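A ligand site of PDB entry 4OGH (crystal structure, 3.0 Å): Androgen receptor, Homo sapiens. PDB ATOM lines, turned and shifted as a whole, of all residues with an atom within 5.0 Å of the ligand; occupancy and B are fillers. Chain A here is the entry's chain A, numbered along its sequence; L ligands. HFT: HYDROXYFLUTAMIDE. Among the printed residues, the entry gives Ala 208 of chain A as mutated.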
ATOM      1  N   LEU A  32      31.670  17.550   6.857  1.00  0.00           N
ATOM      2  CA  LEU A  32      30.223  17.452   7.086  1.00  0.00           C
ATOM      3  C   LEU A  32      29.713  16.043   7.196  1.00  0.00           C
ATOM      4  O   LEU A  32      28.697  15.821   7.834  1.00  0.00           O
ATOM      5  CB  LEU A  32      29.404  18.286   6.113  1.00  0.00           C
ATOM      6  CG  LEU A  32      29.361  19.664   6.803  1.00  0.00           C
ATOM      7  CD1 LEU A  32      29.980  20.748   5.959  1.00  0.00           C
ATOM      8  CD2 LEU A  32      27.987  20.046   7.311  1.00  0.00           C
ATOM      9  N   LEU A  35      30.458  15.598  11.069  1.00  0.00           N
ATOM     10  CA  LEU A  35      29.389  16.328  11.802  1.00  0.00           C
ATOM     11  C   LEU A  35      28.066  15.585  11.821  1.00  0.00           C
ATOM     12  O   LEU A  35      27.426  15.498  12.868  1.00  0.00           O
ATOM     13  CB  LEU A  35      29.136  17.712  11.197  1.00  0.00           C
ATOM     14  CG  LEU A  35      29.942  18.944  11.637  1.00  0.00           C
ATOM     15  CD1 LEU A  35      29.427  20.152  10.869  1.00  0.00           C
ATOM     16  CD2 LEU A  35      29.899  19.195  13.149  1.00  0.00           C
ATOM     17  N   ASN A  36      27.655  15.065  10.649  1.00  0.00           N
ATOM     18  CA  ASN A  36      26.464  14.221  10.525  1.00  0.00           C
ATOM     19  C   ASN A  36      26.580  12.970  11.390  1.00  0.00           C
ATOM     20  O   ASN A  36      25.651  12.621  12.134  1.00  0.00           O
ATOM     21  CB  ASN A  36      26.272  13.790   9.070  1.00  0.00           C
ATOM     22  CG  ASN A  36      25.720  14.885   8.187  1.00  0.00           C
ATOM     23  OD1 ASN A  36      25.316  15.965   8.660  1.00  0.00           O
ATOM     24  ND2 ASN A  36      25.699  14.627   6.881  1.00  0.00           N
ATOM     25  N   LEU A  38      28.406  12.717  13.962  1.00  0.00           N
ATOM     26  CA  LEU A  38      28.366  13.177  15.320  1.00  0.00           C
ATOM     27  C   LEU A  38      26.936  13.483  15.734  1.00  0.00           C
ATOM     28  O   LEU A  38      26.539  13.187  16.877  1.00  0.00           O
ATOM     29  CB  LEU A  38      29.259  14.421  15.469  1.00  0.00           C
ATOM     30  CG  LEU A  38      29.405  15.022  16.856  1.00  0.00           C
ATOM     31  CD1 LEU A  38      29.966  13.933  17.765  1.00  0.00           C
ATOM     32  CD2 LEU A  38      30.289  16.255  16.858  1.00  0.00           C
ATOM     33  N   GLY A  39      26.184  14.067  14.803  1.00  0.00           N
ATOM     34  CA  GLY A  39      24.802  14.455  15.084  1.00  0.00           C
ATOM     35  C   GLY A  39      24.082  13.218  15.592  1.00  0.00           C
ATOM     36  O   GLY A  39      23.533  13.213  16.682  1.00  0.00           O
ATOM     37  N   GLN A  42      25.233  12.047  19.149  1.00  0.00           N
ATOM     38  CA  GLN A  42      24.784  12.946  20.179  1.00  0.00           C
ATOM     39  C   GLN A  42      23.292  12.781  20.316  1.00  0.00           C
ATOM     40  O   GLN A  42      22.764  12.808  21.445  1.00  0.00           O
ATOM     41  CB  GLN A  42      25.189  14.376  19.871  1.00  0.00           C
ATOM     42  CG  GLN A  42      26.663  14.631  20.131  1.00  0.00           C
ATOM     43  CD  GLN A  42      27.042  16.079  19.964  1.00  0.00           C
ATOM     44  OE1 GLN A  42      28.210  16.413  19.936  1.00  0.00           O
ATOM     45  NE2 GLN A  42      26.054  16.945  19.871  1.00  0.00           N
ATOM     46  N   TRP A  72      16.483  18.737  19.751  1.00  0.00           N
ATOM     47  CA  TRP A  72      17.764  18.129  19.529  1.00  0.00           C
ATOM     48  C   TRP A  72      18.879  19.103  19.101  1.00  0.00           C
ATOM     49  O   TRP A  72      19.947  19.104  19.691  1.00  0.00           O
ATOM     50  CB  TRP A  72      17.606  16.920  18.579  1.00  0.00           C
ATOM     51  CG  TRP A  72      18.814  16.557  17.794  1.00  0.00           C
ATOM     52  CD1 TRP A  72      20.013  16.062  18.275  1.00  0.00           C
ATOM     53  CD2 TRP A  72      18.963  16.645  16.369  1.00  0.00           C
ATOM     54  NE1 TRP A  72      20.898  15.839  17.238  1.00  0.00           N
ATOM     55  CE2 TRP A  72      20.277  16.181  16.051  1.00  0.00           C
ATOM     56  CE3 TRP A  72      18.124  17.047  15.309  1.00  0.00           C
ATOM     57  CZ2 TRP A  72      20.779  16.131  14.723  1.00  0.00           C
ATOM     58  CZ3 TRP A  72      18.622  17.003  13.973  1.00  0.00           C
ATOM     59  CH2 TRP A  72      19.931  16.545  13.701  1.00  0.00           C
ATOM     60  N   MET A  73      18.651  19.926  18.103  1.00  0.00           N
ATOM     61  CA  MET A  73      19.753  20.739  17.555  1.00  0.00           C
ATOM     62  C   MET A  73      20.193  21.782  18.547  1.00  0.00           C
ATOM     63  O   MET A  73      21.379  22.063  18.669  1.00  0.00           O
ATOM     64  CB  MET A  73      19.355  21.415  16.242  1.00  0.00           C
ATOM     65  CG  MET A  73      20.450  22.282  15.632  1.00  0.00           C
ATOM     66  SD  MET A  73      21.745  21.283  14.868  1.00  0.00           S
ATOM     67  CE  MET A  73      20.882  20.556  13.466  1.00  0.00           C
ATOM     68  N   MET A  76      22.147  20.279  21.394  1.00  0.00           N
ATOM     69  CA  MET A  76      23.506  20.087  20.909  1.00  0.00           C
ATOM     70  C   MET A  76      24.258  21.433  20.854  1.00  0.00           C
ATOM     71  O   MET A  76      25.413  21.520  21.296  1.00  0.00           O
ATOM     72  CB  MET A  76      23.527  19.422  19.519  1.00  0.00           C
ATOM     73  CG  MET A  76      23.014  17.979  19.463  1.00  0.00           C
ATOM     74  SD  MET A  76      23.604  17.086  17.996  1.00  0.00           S
ATOM     75  CE  MET A  76      23.145  18.191  16.661  1.00  0.00           C
ATOM     76  N   VAL A  77      23.579  22.477  20.344  1.00  0.00           N
ATOM     77  CA  VAL A  77      24.198  23.781  20.229  1.00  0.00           C
ATOM     78  C   VAL A  77      24.652  24.343  21.567  1.00  0.00           C
ATOM     79  O   VAL A  77      25.735  24.926  21.687  1.00  0.00           O
ATOM     80  CB  VAL A  77      23.275  24.785  19.565  1.00  0.00           C
ATOM     81  CG1 VAL A  77      23.825  26.204  19.744  1.00  0.00           C
ATOM     82  CG2 VAL A  77      23.158  24.459  18.085  1.00  0.00           C
ATOM     83  N   MET A  80      27.517  22.173  23.026  1.00  0.00           N
ATOM     84  CA  MET A  80      28.692  22.457  22.229  1.00  0.00           C
ATOM     85  C   MET A  80      29.276  23.806  22.656  1.00  0.00           C
ATOM     86  O   MET A  80      30.483  23.909  22.864  1.00  0.00           O
ATOM     87  CB  MET A  80      28.375  22.382  20.729  1.00  0.00           C
ATOM     88  CG  MET A  80      29.619  22.381  19.844  1.00  0.00           C
ATOM     89  SD  MET A  80      30.352  24.019  19.509  1.00  0.00           S
ATOM     90  CE  MET A  80      29.268  24.678  18.245  1.00  0.00           C
ATOM     91  N   ARG A  83      31.085  23.293  26.160  1.00  0.00           N
ATOM     92  CA  ARG A  83      32.366  22.608  25.910  1.00  0.00           C
ATOM     93  C   ARG A  83      33.347  23.568  25.286  1.00  0.00           C
ATOM     94  O   ARG A  83      34.503  23.591  25.681  1.00  0.00           O
ATOM     95  CB  ARG A  83      32.239  21.474  24.895  1.00  0.00           C
ATOM     96  CG  ARG A  83      31.415  20.283  25.312  1.00  0.00           C
ATOM     97  CD  ARG A  83      31.726  19.133  24.376  1.00  0.00           C
ATOM     98  NE  ARG A  83      31.250  19.357  23.014  1.00  0.00           N
ATOM     99  CZ  ARG A  83      29.977  19.184  22.630  1.00  0.00           C
ATOM    100  NH1 ARG A  83      29.060  18.801  23.516  1.00  0.00           N
ATOM    101  NH2 ARG A  83      29.623  19.402  21.367  1.00  0.00           N
ATOM    102  N   TYR A  94      34.437  23.412  19.879  1.00  0.00           N
ATOM    103  CA  TYR A  94      34.707  22.029  20.295  1.00  0.00           C
ATOM    104  C   TYR A  94      33.498  21.122  20.069  1.00  0.00           C
ATOM    105  O   TYR A  94      32.796  20.707  21.004  1.00  0.00           O
ATOM    106  CB  TYR A  94      35.117  22.043  21.763  1.00  0.00           C
ATOM    107  CG  TYR A  94      35.872  20.831  22.277  1.00  0.00           C
ATOM    108  CD1 TYR A  94      37.246  20.914  22.525  1.00  0.00           C
ATOM    109  CD2 TYR A  94      35.211  19.638  22.580  1.00  0.00           C
ATOM    110  CE1 TYR A  94      37.942  19.829  23.039  1.00  0.00           C
ATOM    111  CE2 TYR A  94      35.893  18.549  23.083  1.00  0.00           C
ATOM    112  CZ  TYR A  94      37.270  18.643  23.313  1.00  0.00           C
ATOM    113  OH  TYR A  94      37.954  17.562  23.822  1.00  0.00           O
ATOM    114  N   PHE A  95      33.231  20.825  18.807  1.00  0.00           N
ATOM    115  CA  PHE A  95      32.198  19.854  18.483  1.00  0.00           C
ATOM    116  C   PHE A  95      32.470  18.516  19.217  1.00  0.00           C
ATOM    117  O   PHE A  95      31.580  17.960  19.850  1.00  0.00           O
ATOM    118  CB  PHE A  95      32.098  19.643  16.972  1.00  0.00           C
ATOM    119  CG  PHE A  95      31.540  20.809  16.220  1.00  0.00           C
ATOM    120  CD1 PHE A  95      32.375  21.676  15.543  1.00  0.00           C
ATOM    121  CD2 PHE A  95      30.176  21.021  16.161  1.00  0.00           C
ATOM    122  CE1 PHE A  95      31.854  22.753  14.829  1.00  0.00           C
ATOM    123  CE2 PHE A  95      29.657  22.085  15.449  1.00  0.00           C
ATOM    124  CZ  PHE A  95      30.492  22.952  14.773  1.00  0.00           C
ATOM    125  N   MET A 118      27.398  30.499  17.021  1.00  0.00           N
ATOM    126  CA  MET A 118      27.699  29.497  18.042  1.00  0.00           C
ATOM    127  C   MET A 118      28.919  29.874  18.855  1.00  0.00           C
ATOM    128  O   MET A 118      28.977  29.595  20.079  1.00  0.00           O
ATOM    129  CB  MET A 118      27.928  28.113  17.422  1.00  0.00           C
ATOM    130  CG  MET A 118      26.651  27.353  17.147  1.00  0.00           C
ATOM    131  SD  MET A 118      26.949  25.829  16.253  1.00  0.00           S
ATOM    132  CE  MET A 118      27.514  26.454  14.654  1.00  0.00           C
ATOM    133  N   LEU A 204      20.814  26.537  11.950  1.00  0.00           N
ATOM    134  CA  LEU A 204      21.390  25.226  11.784  1.00  0.00           C
ATOM    135  C   LEU A 204      20.425  24.274  11.091  1.00  0.00           C
ATOM    136  O   LEU A 204      20.844  23.449  10.244  1.00  0.00           O
ATOM    137  CB  LEU A 204      21.887  24.690  13.125  1.00  0.00           C
ATOM    138  CG  LEU A 204      23.373  25.061  13.279  1.00  0.00           C
ATOM    139  CD1 LEU A 204      23.775  25.022  14.738  1.00  0.00           C
ATOM    140  CD2 LEU A 204      24.289  24.171  12.450  1.00  0.00           C
ATOM    141  N   PHE A 207      20.373  24.966   7.237  1.00  0.00           N
ATOM    142  CA  PHE A 207      21.580  24.393   6.644  1.00  0.00           C
ATOM    143  C   PHE A 207      21.573  22.863   6.507  1.00  0.00           C
ATOM    144  O   PHE A 207      21.972  22.316   5.461  1.00  0.00           O
ATOM    145  CB  PHE A 207      22.827  24.865   7.419  1.00  0.00           C
ATOM    146  CG  PHE A 207      24.092  24.303   6.872  1.00  0.00           C
ATOM    147  CD1 PHE A 207      24.668  23.186   7.456  1.00  0.00           C
ATOM    148  CD2 PHE A 207      24.669  24.863   5.756  1.00  0.00           C
ATOM    149  CE1 PHE A 207      25.836  22.648   6.944  1.00  0.00           C
ATOM    150  CE2 PHE A 207      25.842  24.332   5.233  1.00  0.00           C
ATOM    151  CZ  PHE A 207      26.432  23.218   5.826  1.00  0.00           C
ATOM    152  N   ALA A 208      21.154  22.178   7.569  1.00  0.00           N
ATOM    153  CA  ALA A 208      21.034  20.721   7.560  1.00  0.00           C
ATOM    154  C   ALA A 208      20.045  20.304   6.512  1.00  0.00           C
ATOM    155  O   ALA A 208      20.309  19.390   5.737  1.00  0.00           O
ATOM    156  CB  ALA A 208      20.609  20.186   8.925  1.00  0.00           C
ATOM    157  N   LEU A 211      21.362  20.943   3.022  1.00  0.00           N
ATOM    158  CA  LEU A 211      22.383  19.935   2.831  1.00  0.00           C
ATOM    159  C   LEU A 211      21.787  18.578   2.456  1.00  0.00           C
ATOM    160  O   LEU A 211      22.270  17.956   1.528  1.00  0.00           O
ATOM    161  CB  LEU A 211      23.251  19.804   4.095  1.00  0.00           C
ATOM    162  CG  LEU A 211      24.462  18.902   3.841  1.00  0.00           C
ATOM    163  CD1 LEU A 211      25.201  19.388   2.588  1.00  0.00           C
ATOM    164  CD2 LEU A 211      25.383  18.817   5.062  1.00  0.00           C
ATOM    165  N   MET A 226      19.283  10.460  11.114  1.00  0.00           N
ATOM    166  CA  MET A 226      19.395  11.875  10.731  1.00  0.00           C
ATOM    167  C   MET A 226      18.356  12.214   9.691  1.00  0.00           C
ATOM    168  O   MET A 226      17.407  12.974   9.936  1.00  0.00           O
ATOM    169  CB  MET A 226      20.756  12.145  10.089  1.00  0.00           C
ATOM    170  CG  MET A 226      21.947  12.185  11.002  1.00  0.00           C
ATOM    171  SD  MET A 226      21.885  13.695  11.950  1.00  0.00           S
ATOM    172  CE  MET A 226      20.870  13.150  13.339  1.00  0.00           C
ATOM    173  N   ILE A 230      15.553  15.242   9.681  1.00  0.00           N
ATOM    174  CA  ILE A 230      15.718  16.421   8.861  1.00  0.00           C
ATOM    175  C   ILE A 230      14.605  16.609   7.826  1.00  0.00           C
ATOM    176  O   ILE A 230      14.199  17.736   7.511  1.00  0.00           O
ATOM    177  CB  ILE A 230      17.093  16.420   8.191  1.00  0.00           C
ATOM    178  CG1 ILE A 230      18.185  16.631   9.243  1.00  0.00           C
ATOM    179  CG2 ILE A 230      17.185  17.511   7.133  1.00  0.00           C
ATOM    180  CD1 ILE A 230      19.359  15.681   9.141  1.00  0.00           C
HETATM  181  F1  HFT L   1      25.638  22.432  15.557  1.00  0.00           F
HETATM  182  C7  HFT L   1      26.030  21.740  16.640  1.00  0.00           C
HETATM  183  F2  HFT L   1      25.121  21.777  17.634  1.00  0.00           F
HETATM  184  F3  HFT L   1      27.154  22.247  17.143  1.00  0.00           F
HETATM  185  C3  HFT L   1      26.339  20.331  16.173  1.00  0.00           C
HETATM  186  C2  HFT L   1      25.971  19.982  14.881  1.00  0.00           C
HETATM  187  C4  HFT L   1      27.015  19.294  17.003  1.00  0.00           C
HETATM  188  N1  HFT L   1      27.405  19.524  18.345  1.00  0.00           N
HETATM  189  O2  HFT L   1      28.639  19.156  18.847  1.00  0.00           O
HETATM  190  O1  HFT L   1      26.618  20.023  19.127  1.00  0.00           O
HETATM  191  C5  HFT L   1      27.223  18.038  16.429  1.00  0.00           C
HETATM  192  C6  HFT L   1      26.832  17.748  15.123  1.00  0.00           C
HETATM  193  C1  HFT L   1      26.197  18.707  14.351  1.00  0.00           C
HETATM  194  N9  HFT L   1      25.835  18.403  13.062  1.00  0.00           N
HETATM  195  C10 HFT L   1      25.019  19.173  12.315  1.00  0.00           C
HETATM  196  O10 HFT L   1      24.612  20.261  12.665  1.00  0.00           O
HETATM  197  C11 HFT L   1      24.578  18.723  10.933  1.00  0.00           C
HETATM  198  C12 HFT L   1      23.225  18.006  10.788  1.00  0.00           C
HETATM  199  C13 HFT L   1      25.625  18.738   9.835  1.00  0.00           C
HETATM  200  O11 HFT L   1      25.064  17.401  11.165  1.00  0.00           O
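NE of Arg 83 is in hydrogen-bond range of O of Tyr 94 (2.9 Å). The side-chain sulfur (SD) of Met 76 is in hydrogen-bond range of the indole nitrogen (NE1) of Trp 72, 3.1 Å away. The side-chain sulfur (SD) of Met 76 lies within hydrogen-bond range of the side-chain amide nitrogen (NE2) of Gln 42 (3.1 Å). The side-chain amide nitrogen (ND2) of Asn 36 sits close to the backbone carbonyl oxygen (O) of Leu 32. The guanidinium group (NH2) of Arg 83 lies within hydrogen-bond range of the backbone carbonyl oxygen (O) of Phe 95, 2.9 Å away.
The side-chain sulfur (SD) of Met 73 lies close to an oxygen (O10) of the ligand, at 3.8 Å. The backbone carbonyl oxygen of Met 76 lies close to an oxygen (O1) of the ligand (2.9 Å). A fluorine (F2) of the ligand sits close to the backbone NH (N) of Val 77 (3.2 Å). O of Phe 95 sits close to O2 of the ligand, 3.3 Å away. SD of Met 118 sits close to F3 of the ligand (3.7 Å). CD2 of Leu 32 touches C13 of the ligand, at 3.7 Å. Leu 38 touches the ligand (CD2 to C5, 3.6 Å). Gly 39 touches the ligand (N to C6, 3.8 Å). Met 80 touches the ligand. Leu 204 touches the ligand (CD1 to F1, 3.3 Å). CB of Ala 208 touches C12 of the ligand (3.9 Å). Hydrophobic or aromatic side chains within 4 Å of the ligand: Leu 32, Leu 35, Leu 38, Met 73, Met 76, Val 77, Met 80, Phe 95, Met 118, Leu 204 and Ala 208. Of the 21 residues printed, 15 come within 4 Å of the ligand. Along chain A the residues within 4 Å of the ligand span positions 32 to 208.
OE1 of Gln 42 sits close to O2 of the ligand (3.0 Å). An oxygen (O2) of the ligand is in hydrogen-bond range of the guanidinium group (NH2) of Arg 83 (2.7 Å). The side-chain amide oxygen (OD1) of Asn 36 sits at hydrogen-bond distance from an oxygen (O11) of the ligand, at 2.9 Å. N9 of the ligand lies close to O of Leu 35, at 3.3 Å.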
